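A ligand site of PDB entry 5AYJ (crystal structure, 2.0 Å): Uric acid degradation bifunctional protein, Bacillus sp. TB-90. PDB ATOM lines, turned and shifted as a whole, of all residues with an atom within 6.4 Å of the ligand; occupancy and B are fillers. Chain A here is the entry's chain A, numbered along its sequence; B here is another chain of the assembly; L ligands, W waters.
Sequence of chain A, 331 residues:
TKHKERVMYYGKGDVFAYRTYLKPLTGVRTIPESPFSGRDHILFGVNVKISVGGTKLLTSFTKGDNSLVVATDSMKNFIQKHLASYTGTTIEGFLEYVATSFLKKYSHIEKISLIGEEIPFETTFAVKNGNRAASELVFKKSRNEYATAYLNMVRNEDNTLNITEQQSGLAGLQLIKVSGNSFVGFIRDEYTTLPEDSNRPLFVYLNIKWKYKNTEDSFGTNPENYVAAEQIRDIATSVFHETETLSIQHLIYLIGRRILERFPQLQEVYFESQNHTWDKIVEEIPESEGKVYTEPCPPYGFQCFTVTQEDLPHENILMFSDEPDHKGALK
N of Ile 248 is in hydrogen-bond range of O1 of the ligand (2.6 Å). An oxygen (O1) of the ligand is in hydrogen-bond range of the guanidinium group of Arg 200. OE1 of Gln 249 is in hydrogen-bond range of N1 of the ligand, 2.8 Å away. N of Asp 73 of chain B sits at hydrogen-bond distance from O3 of the ligand (3.1 Å). The backbone NH (N) of Thr 72 of chain B lies within hydrogen-bond range of an oxygen (O3) of the ligand (3.3 Å). A nitrogen (N3) of the ligand lies within hydrogen-bond range of the side-chain hydroxyl of Thr 72 of chain B, at 3.1 Å. N2 of the ligand lies close to ND2 of Asn 275, 3.4 Å away.
The side-chain hydroxyl (OG) of Ser 247 lies close to the backbone NH (N) of Gln 249 (3.2 Å). NZ of Lys 12 of chain B lies within hydrogen-bond range of OG1 of Thr 72 of chain B (3.0 Å). O of Gly 301 sits at hydrogen-bond distance from N of Asn 275 (2.8 Å). O of Val 70 of chain B is in hydrogen-bond range of OH of Tyr 10 of chain B.
Water W1 lies within hydrogen-bond range of OG1 of Thr 72 of chain B (3.3 Å), ND2 of Asn 275 (3.3 Å), NE2 of Gln 303 (3.4 Å) and N3 of the ligand (3.4 Å).
Residues that only touch the ligand: Ser 247, Phe 183, Leu 194, Tyr 10 of chain B, Ala 71 of chain B and Gln 303. Hydrophobic or aromatic side chains within 4 Å of the ligand: Phe 183, Leu 194, Ile 248, Tyr 10 of chain B and Ala 71 of chain B. 12 residues have an atom within 4 Å of the ligand: Phe 183, Leu 194, Arg 200, Ser 247, Ile 248, Gln 249, Asn 275, Gln 303, Tyr 10 of chain B, Ala 71 of chain B, Thr 72 of chain B and Asp 73 of chain B. The nearest printed residue that does not touch the ligand is Val 69 of chain B (4.3 Å).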
ATOM      1  N   SER A 182     -18.580  18.767 -21.980  1.00  0.00           N
ATOM      2  CA  SER A 182     -18.044  20.061 -21.590  1.00  0.00           C
ATOM      3  C   SER A 182     -16.723  19.915 -20.871  1.00  0.00           C
ATOM      4  O   SER A 182     -16.374  18.845 -20.384  1.00  0.00           O
ATOM      5  CB  SER A 182     -19.035  20.824 -20.706  1.00  0.00           C
ATOM      6  OG  SER A 182     -19.088  20.297 -19.401  1.00  0.00           O
ATOM      7  N   PHE A 183     -15.988  21.012 -20.827  1.00  0.00           N
ATOM      8  CA  PHE A 183     -14.818  21.120 -19.967  1.00  0.00           C
ATOM      9  C   PHE A 183     -14.695  22.569 -19.518  1.00  0.00           C
ATOM     10  O   PHE A 183     -14.105  23.407 -20.208  1.00  0.00           O
ATOM     11  CB  PHE A 183     -13.564  20.622 -20.685  1.00  0.00           C
ATOM     12  CG  PHE A 183     -12.367  20.501 -19.783  1.00  0.00           C
ATOM     13  CD1 PHE A 183     -12.398  19.665 -18.679  1.00  0.00           C
ATOM     14  CD2 PHE A 183     -11.219  21.240 -20.020  1.00  0.00           C
ATOM     15  CE1 PHE A 183     -11.298  19.560 -17.842  1.00  0.00           C
ATOM     16  CE2 PHE A 183     -10.135  21.150 -19.195  1.00  0.00           C
ATOM     17  CZ  PHE A 183     -10.165  20.314 -18.101  1.00  0.00           C
ATOM     18  N   LEU A 194      -6.405  27.908 -22.419  1.00  0.00           N
ATOM     19  CA  LEU A 194      -7.511  27.087 -22.866  1.00  0.00           C
ATOM     20  C   LEU A 194      -8.836  27.763 -22.540  1.00  0.00           C
ATOM     21  O   LEU A 194      -9.107  28.069 -21.374  1.00  0.00           O
ATOM     22  CB  LEU A 194      -7.450  25.719 -22.191  1.00  0.00           C
ATOM     23  CG  LEU A 194      -8.526  24.729 -22.631  1.00  0.00           C
ATOM     24  CD1 LEU A 194      -8.242  24.284 -24.055  1.00  0.00           C
ATOM     25  CD2 LEU A 194      -8.624  23.533 -21.666  1.00  0.00           C
ATOM     26  N   ARG A 200     -18.050  20.422 -26.631  1.00  0.00           N
ATOM     27  CA  ARG A 200     -16.936  20.014 -27.484  1.00  0.00           C
ATOM     28  C   ARG A 200     -17.166  18.613 -28.063  1.00  0.00           C
ATOM     29  O   ARG A 200     -17.905  17.823 -27.483  1.00  0.00           O
ATOM     30  CB  ARG A 200     -15.636  20.039 -26.682  1.00  0.00           C
ATOM     31  CG  ARG A 200     -15.590  19.019 -25.557  1.00  0.00           C
ATOM     32  CD  ARG A 200     -14.275  19.098 -24.780  1.00  0.00           C
ATOM     33  NE  ARG A 200     -14.208  18.111 -23.698  1.00  0.00           N
ATOM     34  CZ  ARG A 200     -13.117  17.899 -22.961  1.00  0.00           C
ATOM     35  NH1 ARG A 200     -12.020  18.601 -23.207  1.00  0.00           N
ATOM     36  NH2 ARG A 200     -13.131  16.979 -22.000  1.00  0.00           N
ATOM     37  N   LEU A 202     -15.717  15.499 -27.980  1.00  0.00           N
ATOM     38  CA  LEU A 202     -14.667  14.766 -27.277  1.00  0.00           C
ATOM     39  C   LEU A 202     -14.184  13.500 -28.012  1.00  0.00           C
ATOM     40  O   LEU A 202     -14.965  12.601 -28.338  1.00  0.00           O
ATOM     41  CB  LEU A 202     -15.166  14.399 -25.884  1.00  0.00           C
ATOM     42  CG  LEU A 202     -14.185  13.678 -24.973  1.00  0.00           C
ATOM     43  CD1 LEU A 202     -12.881  14.443 -24.824  1.00  0.00           C
ATOM     44  CD2 LEU A 202     -14.837  13.440 -23.608  1.00  0.00           C
ATOM     45  N   LEU A 246     -18.163  15.771 -18.290  1.00  0.00           N
ATOM     46  CA  LEU A 246     -17.643  17.006 -17.724  1.00  0.00           C
ATOM     47  C   LEU A 246     -16.127  17.076 -17.893  1.00  0.00           C
ATOM     48  O   LEU A 246     -15.530  18.138 -17.690  1.00  0.00           O
ATOM     49  CB  LEU A 246     -18.047  17.084 -16.249  1.00  0.00           C
ATOM     50  CG  LEU A 246     -19.550  17.180 -16.045  1.00  0.00           C
ATOM     51  CD1 LEU A 246     -19.913  16.984 -14.603  1.00  0.00           C
ATOM     52  CD2 LEU A 246     -20.072  18.546 -16.528  1.00  0.00           C
ATOM     53  N   SER A 247     -15.531  15.945 -18.264  1.00  0.00           N
ATOM     54  CA  SER A 247     -14.098  15.806 -18.487  1.00  0.00           C
ATOM     55  C   SER A 247     -13.882  14.375 -18.925  1.00  0.00           C
ATOM     56  O   SER A 247     -14.785  13.558 -18.832  1.00  0.00           O
ATOM     57  CB  SER A 247     -13.282  16.071 -17.224  1.00  0.00           C
ATOM     58  OG  SER A 247     -13.562  15.095 -16.237  1.00  0.00           O
ATOM     59  N   ILE A 248     -12.670  14.042 -19.359  1.00  0.00           N
ATOM     60  CA  ILE A 248     -12.380  12.641 -19.626  1.00  0.00           C
ATOM     61  C   ILE A 248     -12.338  11.903 -18.307  1.00  0.00           C
ATOM     62  O   ILE A 248     -12.706  10.729 -18.240  1.00  0.00           O
ATOM     63  CB  ILE A 248     -11.062  12.452 -20.391  1.00  0.00           C
ATOM     64  CG1 ILE A 248     -11.213  12.999 -21.816  1.00  0.00           C
ATOM     65  CG2 ILE A 248     -10.686  10.962 -20.455  1.00  0.00           C
ATOM     66  CD1 ILE A 248      -9.929  13.062 -22.577  1.00  0.00           C
ATOM     67  N   GLN A 249     -11.878  12.593 -17.270  1.00  0.00           N
ATOM     68  CA  GLN A 249     -11.763  11.994 -15.941  1.00  0.00           C
ATOM     69  C   GLN A 249     -13.116  11.511 -15.475  1.00  0.00           C
ATOM     70  O   GLN A 249     -13.265  10.396 -14.983  1.00  0.00           O
ATOM     71  CB  GLN A 249     -11.201  13.005 -14.930  1.00  0.00           C
ATOM     72  CG  GLN A 249      -9.723  13.306 -15.093  1.00  0.00           C
ATOM     73  CD  GLN A 249      -9.468  14.432 -16.075  1.00  0.00           C
ATOM     74  OE1 GLN A 249     -10.150  14.548 -17.098  1.00  0.00           O
ATOM     75  NE2 GLN A 249      -8.495  15.283 -15.756  1.00  0.00           N
ATOM     76  N   ASN A 275      -6.616  12.160 -24.805  1.00  0.00           N
ATOM     77  CA  ASN A 275      -7.488  13.201 -25.380  1.00  0.00           C
ATOM     78  C   ASN A 275      -6.933  13.690 -26.682  1.00  0.00           C
ATOM     79  O   ASN A 275      -5.864  14.303 -26.699  1.00  0.00           O
ATOM     80  CB  ASN A 275      -7.640  14.400 -24.435  1.00  0.00           C
ATOM     81  CG  ASN A 275      -8.763  15.370 -24.873  1.00  0.00           C
ATOM     82  OD1 ASN A 275      -9.168  15.365 -26.034  1.00  0.00           O
ATOM     83  ND2 ASN A 275      -9.277  16.177 -23.934  1.00  0.00           N
ATOM     84  N   GLY A 301      -3.411  15.088 -24.095  1.00  0.00           N
ATOM     85  CA  GLY A 301      -3.741  14.855 -22.698  1.00  0.00           C
ATOM     86  C   GLY A 301      -3.898  13.356 -22.431  1.00  0.00           C
ATOM     87  O   GLY A 301      -4.288  12.598 -23.318  1.00  0.00           O
ATOM     88  N   PHE A 302      -3.571  12.923 -21.221  1.00  0.00           N
ATOM     89  CA  PHE A 302      -3.885  11.559 -20.821  1.00  0.00           C
ATOM     90  C   PHE A 302      -4.308  11.494 -19.364  1.00  0.00           C
ATOM     91  O   PHE A 302      -4.053  12.390 -18.575  1.00  0.00           O
ATOM     92  CB  PHE A 302      -2.696  10.640 -21.079  1.00  0.00           C
ATOM     93  CG  PHE A 302      -1.484  10.956 -20.258  1.00  0.00           C
ATOM     94  CD1 PHE A 302      -1.320  10.405 -18.993  1.00  0.00           C
ATOM     95  CD2 PHE A 302      -0.522  11.800 -20.754  1.00  0.00           C
ATOM     96  CE1 PHE A 302      -0.225  10.699 -18.244  1.00  0.00           C
ATOM     97  CE2 PHE A 302       0.580  12.106 -20.006  1.00  0.00           C
ATOM     98  CZ  PHE A 302       0.747  11.546 -18.750  1.00  0.00           C
ATOM     99  N   GLN A 303      -5.009  10.415 -19.047  1.00  0.00           N
ATOM    100  CA  GLN A 303      -5.564  10.168 -17.738  1.00  0.00           C
ATOM    101  C   GLN A 303      -5.304   8.705 -17.427  1.00  0.00           C
ATOM    102  O   GLN A 303      -5.345   7.832 -18.310  1.00  0.00           O
ATOM    103  CB  GLN A 303      -7.070  10.484 -17.716  1.00  0.00           C
ATOM    104  CG  GLN A 303      -7.435  11.946 -17.940  1.00  0.00           C
ATOM    105  CD  GLN A 303      -7.290  12.412 -19.386  1.00  0.00           C
ATOM    106  OE1 GLN A 303      -7.395  11.617 -20.340  1.00  0.00           O
ATOM    107  NE2 GLN A 303      -7.029  13.701 -19.549  1.00  0.00           N
ATOM    108  N   TYR B  10      -2.785  12.124 -14.227  1.00  0.00           N
ATOM    109  CA  TYR B  10      -3.139  12.653 -15.548  1.00  0.00           C
ATOM    110  C   TYR B  10      -2.042  13.633 -15.941  1.00  0.00           C
ATOM    111  O   TYR B  10      -1.276  14.079 -15.099  1.00  0.00           O
ATOM    112  CB  TYR B  10      -4.521  13.319 -15.545  1.00  0.00           C
ATOM    113  CG  TYR B  10      -4.567  14.738 -15.009  1.00  0.00           C
ATOM    114  CD1 TYR B  10      -4.266  15.012 -13.686  1.00  0.00           C
ATOM    115  CD2 TYR B  10      -4.922  15.803 -15.828  1.00  0.00           C
ATOM    116  CE1 TYR B  10      -4.305  16.302 -13.187  1.00  0.00           C
ATOM    117  CE2 TYR B  10      -4.954  17.105 -15.340  1.00  0.00           C
ATOM    118  CZ  TYR B  10      -4.644  17.351 -14.014  1.00  0.00           C
ATOM    119  OH  TYR B  10      -4.662  18.640 -13.485  1.00  0.00           O
ATOM    120  N   GLY B  11      -1.964  13.938 -17.234  1.00  0.00           N
ATOM    121  CA  GLY B  11      -0.993  14.892 -17.709  1.00  0.00           C
ATOM    122  C   GLY B  11      -0.983  15.080 -19.215  1.00  0.00           C
ATOM    123  O   GLY B  11      -1.998  14.936 -19.874  1.00  0.00           O
ATOM    124  N   LYS B  12       0.194  15.388 -19.741  1.00  0.00           N
ATOM    125  CA  LYS B  12       0.369  15.754 -21.126  1.00  0.00           C
ATOM    126  C   LYS B  12       1.586  15.061 -21.697  1.00  0.00           C
ATOM    127  O   LYS B  12       2.656  15.060 -21.082  1.00  0.00           O
ATOM    128  CB  LYS B  12       0.551  17.266 -21.244  1.00  0.00           C
ATOM    129  CG  LYS B  12       0.279  17.834 -22.625  1.00  0.00           C
ATOM    130  CD  LYS B  12      -1.196  17.781 -22.899  1.00  0.00           C
ATOM    131  CE  LYS B  12      -1.660  18.899 -23.798  1.00  0.00           C
ATOM    132  NZ  LYS B  12      -3.120  18.860 -23.891  1.00  0.00           N
ATOM    133  N   ASN B  66     -14.067  20.290 -11.595  1.00  0.00           N
ATOM    134  CA  ASN B  66     -12.785  20.630 -12.211  1.00  0.00           C
ATOM    135  C   ASN B  66     -12.020  21.705 -11.480  1.00  0.00           C
ATOM    136  O   ASN B  66     -10.975  22.137 -11.943  1.00  0.00           O
ATOM    137  CB  ASN B  66     -13.021  21.045 -13.657  1.00  0.00           C
ATOM    138  CG  ASN B  66     -13.358  19.871 -14.554  1.00  0.00           C
ATOM    139  OD1 ASN B  66     -12.829  18.769 -14.368  1.00  0.00           O
ATOM    140  ND2 ASN B  66     -14.230  20.094 -15.514  1.00  0.00           N
ATOM    141  N   VAL B  69      -8.417  21.104 -11.021  1.00  0.00           N
ATOM    142  CA  VAL B  69      -7.774  20.603 -12.215  1.00  0.00           C
ATOM    143  C   VAL B  69      -6.920  21.676 -12.917  1.00  0.00           C
ATOM    144  O   VAL B  69      -7.423  22.732 -13.309  1.00  0.00           O
ATOM    145  CB  VAL B  69      -8.808  20.049 -13.207  1.00  0.00           C
ATOM    146  CG1 VAL B  69      -8.136  19.630 -14.498  1.00  0.00           C
ATOM    147  CG2 VAL B  69      -9.575  18.899 -12.585  1.00  0.00           C
ATOM    148  N   VAL B  70      -5.634  21.398 -13.042  1.00  0.00           N
ATOM    149  CA  VAL B  70      -4.738  22.127 -13.941  1.00  0.00           C
ATOM    150  C   VAL B  70      -4.956  21.546 -15.322  1.00  0.00           C
ATOM    151  O   VAL B  70      -4.790  20.345 -15.532  1.00  0.00           O
ATOM    152  CB  VAL B  70      -3.264  22.006 -13.521  1.00  0.00           C
ATOM    153  CG1 VAL B  70      -2.339  22.714 -14.507  1.00  0.00           C
ATOM    154  CG2 VAL B  70      -3.064  22.543 -12.106  1.00  0.00           C
ATOM    155  N   ALA B  71      -5.375  22.380 -16.262  1.00  0.00           N
ATOM    156  CA  ALA B  71      -5.627  21.908 -17.614  1.00  0.00           C
ATOM    157  C   ALA B  71      -4.306  21.321 -18.170  1.00  0.00           C
ATOM    158  O   ALA B  71      -3.228  21.861 -17.919  1.00  0.00           O
ATOM    159  CB  ALA B  71      -6.132  23.026 -18.495  1.00  0.00           C
ATOM    160  N   THR B  72      -4.380  20.205 -18.881  1.00  0.00           N
ATOM    161  CA  THR B  72      -3.165  19.589 -19.408  1.00  0.00           C
ATOM    162  C   THR B  72      -2.582  20.566 -20.444  1.00  0.00           C
ATOM    163  O   THR B  72      -1.376  20.624 -20.644  1.00  0.00           O
ATOM    164  CB  THR B  72      -3.420  18.168 -20.006  1.00  0.00           C
ATOM    165  OG1 THR B  72      -4.273  18.262 -21.144  1.00  0.00           O
ATOM    166  CG2 THR B  72      -4.056  17.228 -18.966  1.00  0.00           C
ATOM    167  N   ASP B  73      -3.447  21.376 -21.047  1.00  0.00           N
ATOM    168  CA  ASP B  73      -2.965  22.408 -21.972  1.00  0.00           C
ATOM    169  C   ASP B  73      -2.073  23.407 -21.218  1.00  0.00           C
ATOM    170  O   ASP B  73      -1.059  23.907 -21.749  1.00  0.00           O
ATOM    171  CB  ASP B  73      -4.135  23.121 -22.618  1.00  0.00           C
ATOM    172  CG  ASP B  73      -3.681  24.178 -23.626  1.00  0.00           C
ATOM    173  OD1 ASP B  73      -3.337  23.803 -24.763  1.00  0.00           O
ATOM    174  OD2 ASP B  73      -3.681  25.379 -23.288  1.00  0.00           O
ATOM    175  N   SER B  74      -2.428  23.677 -19.961  1.00  0.00           N
ATOM    176  CA  SER B  74      -1.708  24.659 -19.182  1.00  0.00           C
ATOM    177  C   SER B  74      -0.357  24.078 -18.793  1.00  0.00           C
ATOM    178  O   SER B  74       0.622  24.811 -18.714  1.00  0.00           O
ATOM    179  CB  SER B  74      -2.505  25.077 -17.946  1.00  0.00           C
ATOM    180  OG  SER B  74      -3.777  25.601 -18.307  1.00  0.00           O
HETATM  181  N1  LIG L   1      -9.509  16.540 -19.012  1.00  0.00           N
HETATM  182  C1  LIG L   1     -10.355  16.782 -20.063  1.00  0.00           C
HETATM  183  O1  LIG L   1     -11.371  16.139 -20.182  1.00  0.00           O
HETATM  184  N2  LIG L   1     -10.037  17.734 -20.986  1.00  0.00           N
HETATM  185  C2  LIG L   1      -8.891  18.467 -20.881  1.00  0.00           C
HETATM  186  C3  LIG L   1      -8.087  18.223 -19.831  1.00  0.00           C
HETATM  187  C4  LIG L   1      -8.390  17.257 -18.886  1.00  0.00           C
HETATM  188  O2  LIG L   1      -7.656  17.043 -17.942  1.00  0.00           O
HETATM  189  N3  LIG L   1      -7.046  19.071 -19.932  1.00  0.00           N
HETATM  190  C5  LIG L   1      -7.182  19.835 -21.036  1.00  0.00           C
HETATM  191  N4  LIG L   1      -8.336  19.457 -21.627  1.00  0.00           N
HETATM  192  C6  LIG L   1      -8.872  20.029 -22.819  1.00  0.00           C
HETATM  193  O3  LIG L   1      -6.417  20.707 -21.411  1.00  0.00           O
HETATM  194  O   HOH W   1      -6.751  16.214 -21.759  1.00  0.00           O
HETATM  195  O   HOH W   2     -10.659  19.610 -25.733  1.00  0.00           O
